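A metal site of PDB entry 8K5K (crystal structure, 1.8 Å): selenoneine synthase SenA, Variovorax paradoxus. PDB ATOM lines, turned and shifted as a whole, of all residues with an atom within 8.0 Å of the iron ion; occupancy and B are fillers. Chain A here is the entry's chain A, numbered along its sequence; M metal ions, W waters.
Within 4 Å of the iron ion: His 82, His 178 and His 182.
Along chain A the residues within 4 Å of the iron ion span positions 82 to 182.
The iron ion is bound by a ring nitrogen (NE2) of His 178 (2.0 Å), a ring nitrogen (NE2) of His 182 (2.1 Å), a ring nitrogen (NE2) of His 82 (2.1 Å), water W3 (2.2 Å), water W1 (2.3 Å) and water W2 (2.3 Å).
The iron ion has six donor atoms within binding distance.
A ring nitrogen (ND1) of His 182 is in hydrogen-bond range of the side-chain carboxylate (OE2) of Glu 79 (2.7 Å).
The backbone carbonyl oxygen (O) of Tyr 121 sits at hydrogen-bond distance from a ring nitrogen (ND1) of His 82 (2.7 Å).
Water W2 lies within hydrogen-bond range of OH of Tyr 374 and OG of Ser 123.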
ATOM      1  N   ASN A  74      30.548 -17.799 -12.518  1.00  0.00           N
ATOM      2  CA  ASN A  74      31.413 -18.010 -13.701  1.00  0.00           C
ATOM      3  C   ASN A  74      31.445 -16.673 -14.430  1.00  0.00           C
ATOM      4  O   ASN A  74      30.457 -15.928 -14.414  1.00  0.00           O
ATOM      5  CB  ASN A  74      30.936 -19.118 -14.645  1.00  0.00           C
ATOM      6  CG  ASN A  74      31.009 -20.529 -14.051  1.00  0.00           C
ATOM      7  OD1 ASN A  74      32.088 -21.060 -13.771  1.00  0.00           O
ATOM      8  ND2 ASN A  74      29.848 -21.128 -13.888  1.00  0.00           N
ATOM      9  N   TRP A  78      32.247 -16.519 -20.428  1.00  0.00           N
ATOM     10  CA  TRP A  78      32.437 -17.991 -20.343  1.00  0.00           C
ATOM     11  C   TRP A  78      31.058 -18.667 -20.399  1.00  0.00           C
ATOM     12  O   TRP A  78      30.881 -19.574 -21.201  1.00  0.00           O
ATOM     13  CB  TRP A  78      33.199 -18.386 -19.068  1.00  0.00           C
ATOM     14  CG  TRP A  78      33.474 -19.855 -19.112  1.00  0.00           C
ATOM     15  CD1 TRP A  78      34.539 -20.466 -19.682  1.00  0.00           C
ATOM     16  CD2 TRP A  78      32.608 -20.893 -18.652  1.00  0.00           C
ATOM     17  NE1 TRP A  78      34.413 -21.818 -19.592  1.00  0.00           N
ATOM     18  CE2 TRP A  78      33.255 -22.111 -18.929  1.00  0.00           C
ATOM     19  CE3 TRP A  78      31.384 -20.915 -17.965  1.00  0.00           C
ATOM     20  CZ2 TRP A  78      32.695 -23.338 -18.622  1.00  0.00           C
ATOM     21  CZ3 TRP A  78      30.829 -22.134 -17.657  1.00  0.00           C
ATOM     22  CH2 TRP A  78      31.488 -23.332 -17.963  1.00  0.00           C
ATOM     23  N   GLU A  79      30.108 -18.198 -19.608  1.00  0.00           N
ATOM     24  CA  GLU A  79      28.703 -18.707 -19.614  1.00  0.00           C
ATOM     25  C   GLU A  79      28.130 -18.701 -21.036  1.00  0.00           C
ATOM     26  O   GLU A  79      27.539 -19.706 -21.453  1.00  0.00           O
ATOM     27  CB  GLU A  79      27.823 -17.858 -18.681  1.00  0.00           C
ATOM     28  CG  GLU A  79      28.093 -18.119 -17.213  1.00  0.00           C
ATOM     29  CD  GLU A  79      27.456 -19.375 -16.686  1.00  0.00           C
ATOM     30  OE1 GLU A  79      28.169 -20.129 -16.043  1.00  0.00           O
ATOM     31  OE2 GLU A  79      26.237 -19.632 -16.978  1.00  0.00           O
ATOM     32  N   HIS A  82      29.827 -21.241 -23.181  1.00  0.00           N
ATOM     33  CA  HIS A  82      29.418 -22.569 -22.676  1.00  0.00           C
ATOM     34  C   HIS A  82      28.034 -22.949 -23.226  1.00  0.00           C
ATOM     35  O   HIS A  82      27.800 -24.154 -23.537  1.00  0.00           O
ATOM     36  CB  HIS A  82      29.526 -22.637 -21.150  1.00  0.00           C
ATOM     37  CG  HIS A  82      28.869 -23.873 -20.610  1.00  0.00           C
ATOM     38  ND1 HIS A  82      29.488 -25.126 -20.647  1.00  0.00           N
ATOM     39  CD2 HIS A  82      27.674 -24.048 -20.016  1.00  0.00           C
ATOM     40  CE1 HIS A  82      28.644 -26.032 -20.148  1.00  0.00           C
ATOM     41  NE2 HIS A  82      27.538 -25.386 -19.694  1.00  0.00           N
ATOM     42  N   VAL A  83      27.102 -21.997 -23.293  1.00  0.00           N
ATOM     43  CA  VAL A  83      25.730 -22.259 -23.828  1.00  0.00           C
ATOM     44  C   VAL A  83      25.842 -22.746 -25.290  1.00  0.00           C
ATOM     45  O   VAL A  83      25.260 -23.784 -25.657  1.00  0.00           O
ATOM     46  CB  VAL A  83      24.812 -21.034 -23.657  1.00  0.00           C
ATOM     47  CG1 VAL A  83      23.560 -21.153 -24.525  1.00  0.00           C
ATOM     48  CG2 VAL A  83      24.408 -20.859 -22.193  1.00  0.00           C
ATOM     49  N   TRP A  85      28.619 -23.965 -26.760  1.00  0.00           N
ATOM     50  CA  TRP A  85      29.415 -25.225 -26.759  1.00  0.00           C
ATOM     51  C   TRP A  85      28.500 -26.421 -26.476  1.00  0.00           C
ATOM     52  O   TRP A  85      28.576 -27.416 -27.182  1.00  0.00           O
ATOM     53  CB  TRP A  85      30.583 -25.165 -25.779  1.00  0.00           C
ATOM     54  CG  TRP A  85      31.189 -26.527 -25.595  1.00  0.00           C
ATOM     55  CD1 TRP A  85      32.176 -27.076 -26.352  1.00  0.00           C
ATOM     56  CD2 TRP A  85      30.801 -27.531 -24.638  1.00  0.00           C
ATOM     57  NE1 TRP A  85      32.441 -28.353 -25.933  1.00  0.00           N
ATOM     58  CE2 TRP A  85      31.631 -28.657 -24.874  1.00  0.00           C
ATOM     59  CE3 TRP A  85      29.912 -27.579 -23.569  1.00  0.00           C
ATOM     60  CZ2 TRP A  85      31.558 -29.818 -24.102  1.00  0.00           C
ATOM     61  CZ3 TRP A  85      29.822 -28.740 -22.815  1.00  0.00           C
ATOM     62  CH2 TRP A  85      30.622 -29.846 -23.096  1.00  0.00           C
ATOM     63  N   PHE A  86      27.670 -26.327 -25.440  1.00  0.00           N
ATOM     64  CA  PHE A  86      26.755 -27.414 -25.016  1.00  0.00           C
ATOM     65  C   PHE A  86      25.815 -27.745 -26.163  1.00  0.00           C
ATOM     66  O   PHE A  86      25.562 -28.943 -26.450  1.00  0.00           O
ATOM     67  CB  PHE A  86      25.981 -27.032 -23.760  1.00  0.00           C
ATOM     68  CG  PHE A  86      25.203 -28.154 -23.161  1.00  0.00           C
ATOM     69  CD1 PHE A  86      23.883 -28.379 -23.571  1.00  0.00           C
ATOM     70  CD2 PHE A  86      25.742 -28.948 -22.151  1.00  0.00           C
ATOM     71  CE1 PHE A  86      23.145 -29.393 -23.008  1.00  0.00           C
ATOM     72  CE2 PHE A  86      24.991 -29.976 -21.604  1.00  0.00           C
ATOM     73  CZ  PHE A  86      23.688 -30.185 -22.030  1.00  0.00           C
ATOM     74  N   TYR A 121      35.210 -24.643 -22.774  1.00  0.00           N
ATOM     75  CA  TYR A 121      33.785 -24.503 -22.397  1.00  0.00           C
ATOM     76  C   TYR A 121      33.195 -25.769 -21.796  1.00  0.00           C
ATOM     77  O   TYR A 121      32.059 -25.690 -21.311  1.00  0.00           O
ATOM     78  CB  TYR A 121      32.963 -24.059 -23.613  1.00  0.00           C
ATOM     79  CG  TYR A 121      33.342 -22.720 -24.175  1.00  0.00           C
ATOM     80  CD1 TYR A 121      33.319 -21.566 -23.409  1.00  0.00           C
ATOM     81  CD2 TYR A 121      33.675 -22.599 -25.511  1.00  0.00           C
ATOM     82  CE1 TYR A 121      33.611 -20.320 -23.952  1.00  0.00           C
ATOM     83  CE2 TYR A 121      33.995 -21.377 -26.063  1.00  0.00           C
ATOM     84  CZ  TYR A 121      33.946 -20.235 -25.285  1.00  0.00           C
ATOM     85  OH  TYR A 121      34.252 -19.079 -25.890  1.00  0.00           O
ATOM     86  N   ASP A 122      33.870 -26.918 -21.908  1.00  0.00           N
ATOM     87  CA  ASP A 122      33.298 -28.164 -21.377  1.00  0.00           C
ATOM     88  C   ASP A 122      33.332 -28.090 -19.861  1.00  0.00           C
ATOM     89  O   ASP A 122      34.434 -28.100 -19.266  1.00  0.00           O
ATOM     90  CB  ASP A 122      34.042 -29.376 -21.973  1.00  0.00           C
ATOM     91  CG  ASP A 122      33.559 -30.725 -21.441  1.00  0.00           C
ATOM     92  OD1 ASP A 122      32.863 -30.733 -20.419  1.00  0.00           O
ATOM     93  OD2 ASP A 122      33.922 -31.723 -22.045  1.00  0.00           O
ATOM     94  N   SER A 123      32.153 -27.948 -19.226  1.00  0.00           N
ATOM     95  CA  SER A 123      32.079 -27.709 -17.757  1.00  0.00           C
ATOM     96  C   SER A 123      32.616 -28.939 -16.999  1.00  0.00           C
ATOM     97  O   SER A 123      32.942 -28.789 -15.818  1.00  0.00           O
ATOM     98  CB  SER A 123      30.686 -27.314 -17.371  1.00  0.00           C
ATOM     99  OG  SER A 123      29.754 -28.315 -17.738  1.00  0.00           O
ATOM    100  N   GLY A 124      32.709 -30.097 -17.650  1.00  0.00           N
ATOM    101  CA  GLY A 124      33.256 -31.356 -17.089  1.00  0.00           C
ATOM    102  C   GLY A 124      34.777 -31.411 -17.157  1.00  0.00           C
ATOM    103  O   GLY A 124      35.376 -32.268 -16.473  1.00  0.00           O
ATOM    104  N   ARG A 131      38.538 -20.701 -15.472  1.00  0.00           N
ATOM    105  CA  ARG A 131      37.551 -20.069 -16.382  1.00  0.00           C
ATOM    106  C   ARG A 131      37.775 -18.557 -16.428  1.00  0.00           C
ATOM    107  O   ARG A 131      37.242 -17.924 -17.354  1.00  0.00           O
ATOM    108  CB  ARG A 131      36.126 -20.368 -15.931  1.00  0.00           C
ATOM    109  CG  ARG A 131      35.785 -21.850 -16.000  1.00  0.00           C
ATOM    110  CD  ARG A 131      34.472 -22.185 -15.350  1.00  0.00           C
ATOM    111  NE  ARG A 131      34.323 -23.638 -15.367  1.00  0.00           N
ATOM    112  CZ  ARG A 131      33.212 -24.294 -15.029  1.00  0.00           C
ATOM    113  NH1 ARG A 131      32.145 -23.641 -14.625  1.00  0.00           N
ATOM    114  NH2 ARG A 131      33.192 -25.617 -15.083  1.00  0.00           N
ATOM    115  N   HIS A 178      18.839 -26.781 -20.999  1.00  0.00           N
ATOM    116  CA  HIS A 178      20.177 -26.435 -20.443  1.00  0.00           C
ATOM    117  C   HIS A 178      20.345 -24.923 -20.531  1.00  0.00           C
ATOM    118  O   HIS A 178      20.803 -24.306 -19.569  1.00  0.00           O
ATOM    119  CB  HIS A 178      21.303 -27.098 -21.243  1.00  0.00           C
ATOM    120  CG  HIS A 178      22.669 -26.634 -20.848  1.00  0.00           C
ATOM    121  ND1 HIS A 178      23.406 -25.773 -21.665  1.00  0.00           N
ATOM    122  CD2 HIS A 178      23.455 -26.982 -19.817  1.00  0.00           C
ATOM    123  CE1 HIS A 178      24.596 -25.589 -21.098  1.00  0.00           C
ATOM    124  NE2 HIS A 178      24.665 -26.318 -19.977  1.00  0.00           N
ATOM    125  N   GLU A 179      19.924 -24.328 -21.648  1.00  0.00           N
ATOM    126  CA  GLU A 179      20.094 -22.891 -21.891  1.00  0.00           C
ATOM    127  C   GLU A 179      19.164 -22.120 -20.948  1.00  0.00           C
ATOM    128  O   GLU A 179      19.603 -21.059 -20.424  1.00  0.00           O
ATOM    129  CB  GLU A 179      19.923 -22.592 -23.366  1.00  0.00           C
ATOM    130  CG  GLU A 179      20.000 -21.090 -23.651  1.00  0.00           C
ATOM    131  CD  GLU A 179      20.177 -20.736 -25.114  1.00  0.00           C
ATOM    132  OE1 GLU A 179      20.224 -19.523 -25.427  1.00  0.00           O
ATOM    133  OE2 GLU A 179      20.335 -21.649 -25.925  1.00  0.00           O
ATOM    134  N   MET A 181      18.432 -23.150 -17.924  1.00  0.00           N
ATOM    135  CA  MET A 181      19.131 -23.221 -16.618  1.00  0.00           C
ATOM    136  C   MET A 181      20.208 -22.153 -16.514  1.00  0.00           C
ATOM    137  O   MET A 181      20.238 -21.464 -15.500  1.00  0.00           O
ATOM    138  CB  MET A 181      19.776 -24.586 -16.387  1.00  0.00           C
ATOM    139  CG  MET A 181      18.775 -25.688 -16.232  1.00  0.00           C
ATOM    140  SD  MET A 181      19.729 -27.245 -16.249  1.00  0.00           S
ATOM    141  CE  MET A 181      18.365 -28.375 -16.482  1.00  0.00           C
ATOM    142  N   HIS A 182      21.005 -21.945 -17.558  1.00  0.00           N
ATOM    143  CA  HIS A 182      22.101 -20.957 -17.546  1.00  0.00           C
ATOM    144  C   HIS A 182      21.503 -19.544 -17.516  1.00  0.00           C
ATOM    145  O   HIS A 182      22.067 -18.711 -16.845  1.00  0.00           O
ATOM    146  CB  HIS A 182      23.059 -21.219 -18.698  1.00  0.00           C
ATOM    147  CG  HIS A 182      24.017 -22.316 -18.380  1.00  0.00           C
ATOM    148  ND1 HIS A 182      25.160 -22.067 -17.653  1.00  0.00           N
ATOM    149  CD2 HIS A 182      23.977 -23.642 -18.615  1.00  0.00           C
ATOM    150  CE1 HIS A 182      25.832 -23.200 -17.487  1.00  0.00           C
ATOM    151  NE2 HIS A 182      25.131 -24.195 -18.088  1.00  0.00           N
ATOM    152  N   TYR A 374      24.035 -36.913 -20.877  1.00  0.00           N
ATOM    153  CA  TYR A 374      24.735 -35.897 -20.052  1.00  0.00           C
ATOM    154  C   TYR A 374      24.907 -36.475 -18.635  1.00  0.00           C
ATOM    155  O   TYR A 374      24.089 -36.182 -17.701  1.00  0.00           O
ATOM    156  CB  TYR A 374      23.989 -34.564 -20.126  1.00  0.00           C
ATOM    157  CG  TYR A 374      24.507 -33.431 -19.298  1.00  0.00           C
ATOM    158  CD1 TYR A 374      25.823 -33.378 -18.851  1.00  0.00           C
ATOM    159  CD2 TYR A 374      23.681 -32.374 -18.967  1.00  0.00           C
ATOM    160  CE1 TYR A 374      26.294 -32.314 -18.089  1.00  0.00           C
ATOM    161  CE2 TYR A 374      24.131 -31.297 -18.225  1.00  0.00           C
ATOM    162  CZ  TYR A 374      25.446 -31.254 -17.789  1.00  0.00           C
ATOM    163  OH  TYR A 374      25.902 -30.188 -17.075  1.00  0.00           O
ATOM    164  N   TYR A 377      24.935 -34.717 -15.072  1.00  0.00           N
ATOM    165  CA  TYR A 377      23.855 -33.769 -14.701  1.00  0.00           C
ATOM    166  C   TYR A 377      23.393 -34.005 -13.253  1.00  0.00           C
ATOM    167  O   TYR A 377      23.239 -33.026 -12.447  1.00  0.00           O
ATOM    168  CB  TYR A 377      22.689 -33.759 -15.709  1.00  0.00           C
ATOM    169  CG  TYR A 377      21.587 -32.816 -15.293  1.00  0.00           C
ATOM    170  CD1 TYR A 377      21.770 -31.430 -15.245  1.00  0.00           C
ATOM    171  CD2 TYR A 377      20.377 -33.314 -14.890  1.00  0.00           C
ATOM    172  CE1 TYR A 377      20.774 -30.583 -14.778  1.00  0.00           C
ATOM    173  CE2 TYR A 377      19.349 -32.490 -14.465  1.00  0.00           C
ATOM    174  CZ  TYR A 377      19.550 -31.120 -14.366  1.00  0.00           C
ATOM    175  OH  TYR A 377      18.534 -30.327 -13.923  1.00  0.00           O
HETATM  176 FE    FE M   1      25.954 -26.066 -18.439  1.00  0.00          FE
HETATM  177  O   HOH W   1      24.656 -26.917 -16.797  1.00  0.00           O
HETATM  178  O   HOH W   2      26.679 -28.235 -18.703  1.00  0.00           O
HETATM  179  O   HOH W   3      27.220 -26.124 -16.665  1.00  0.00           O
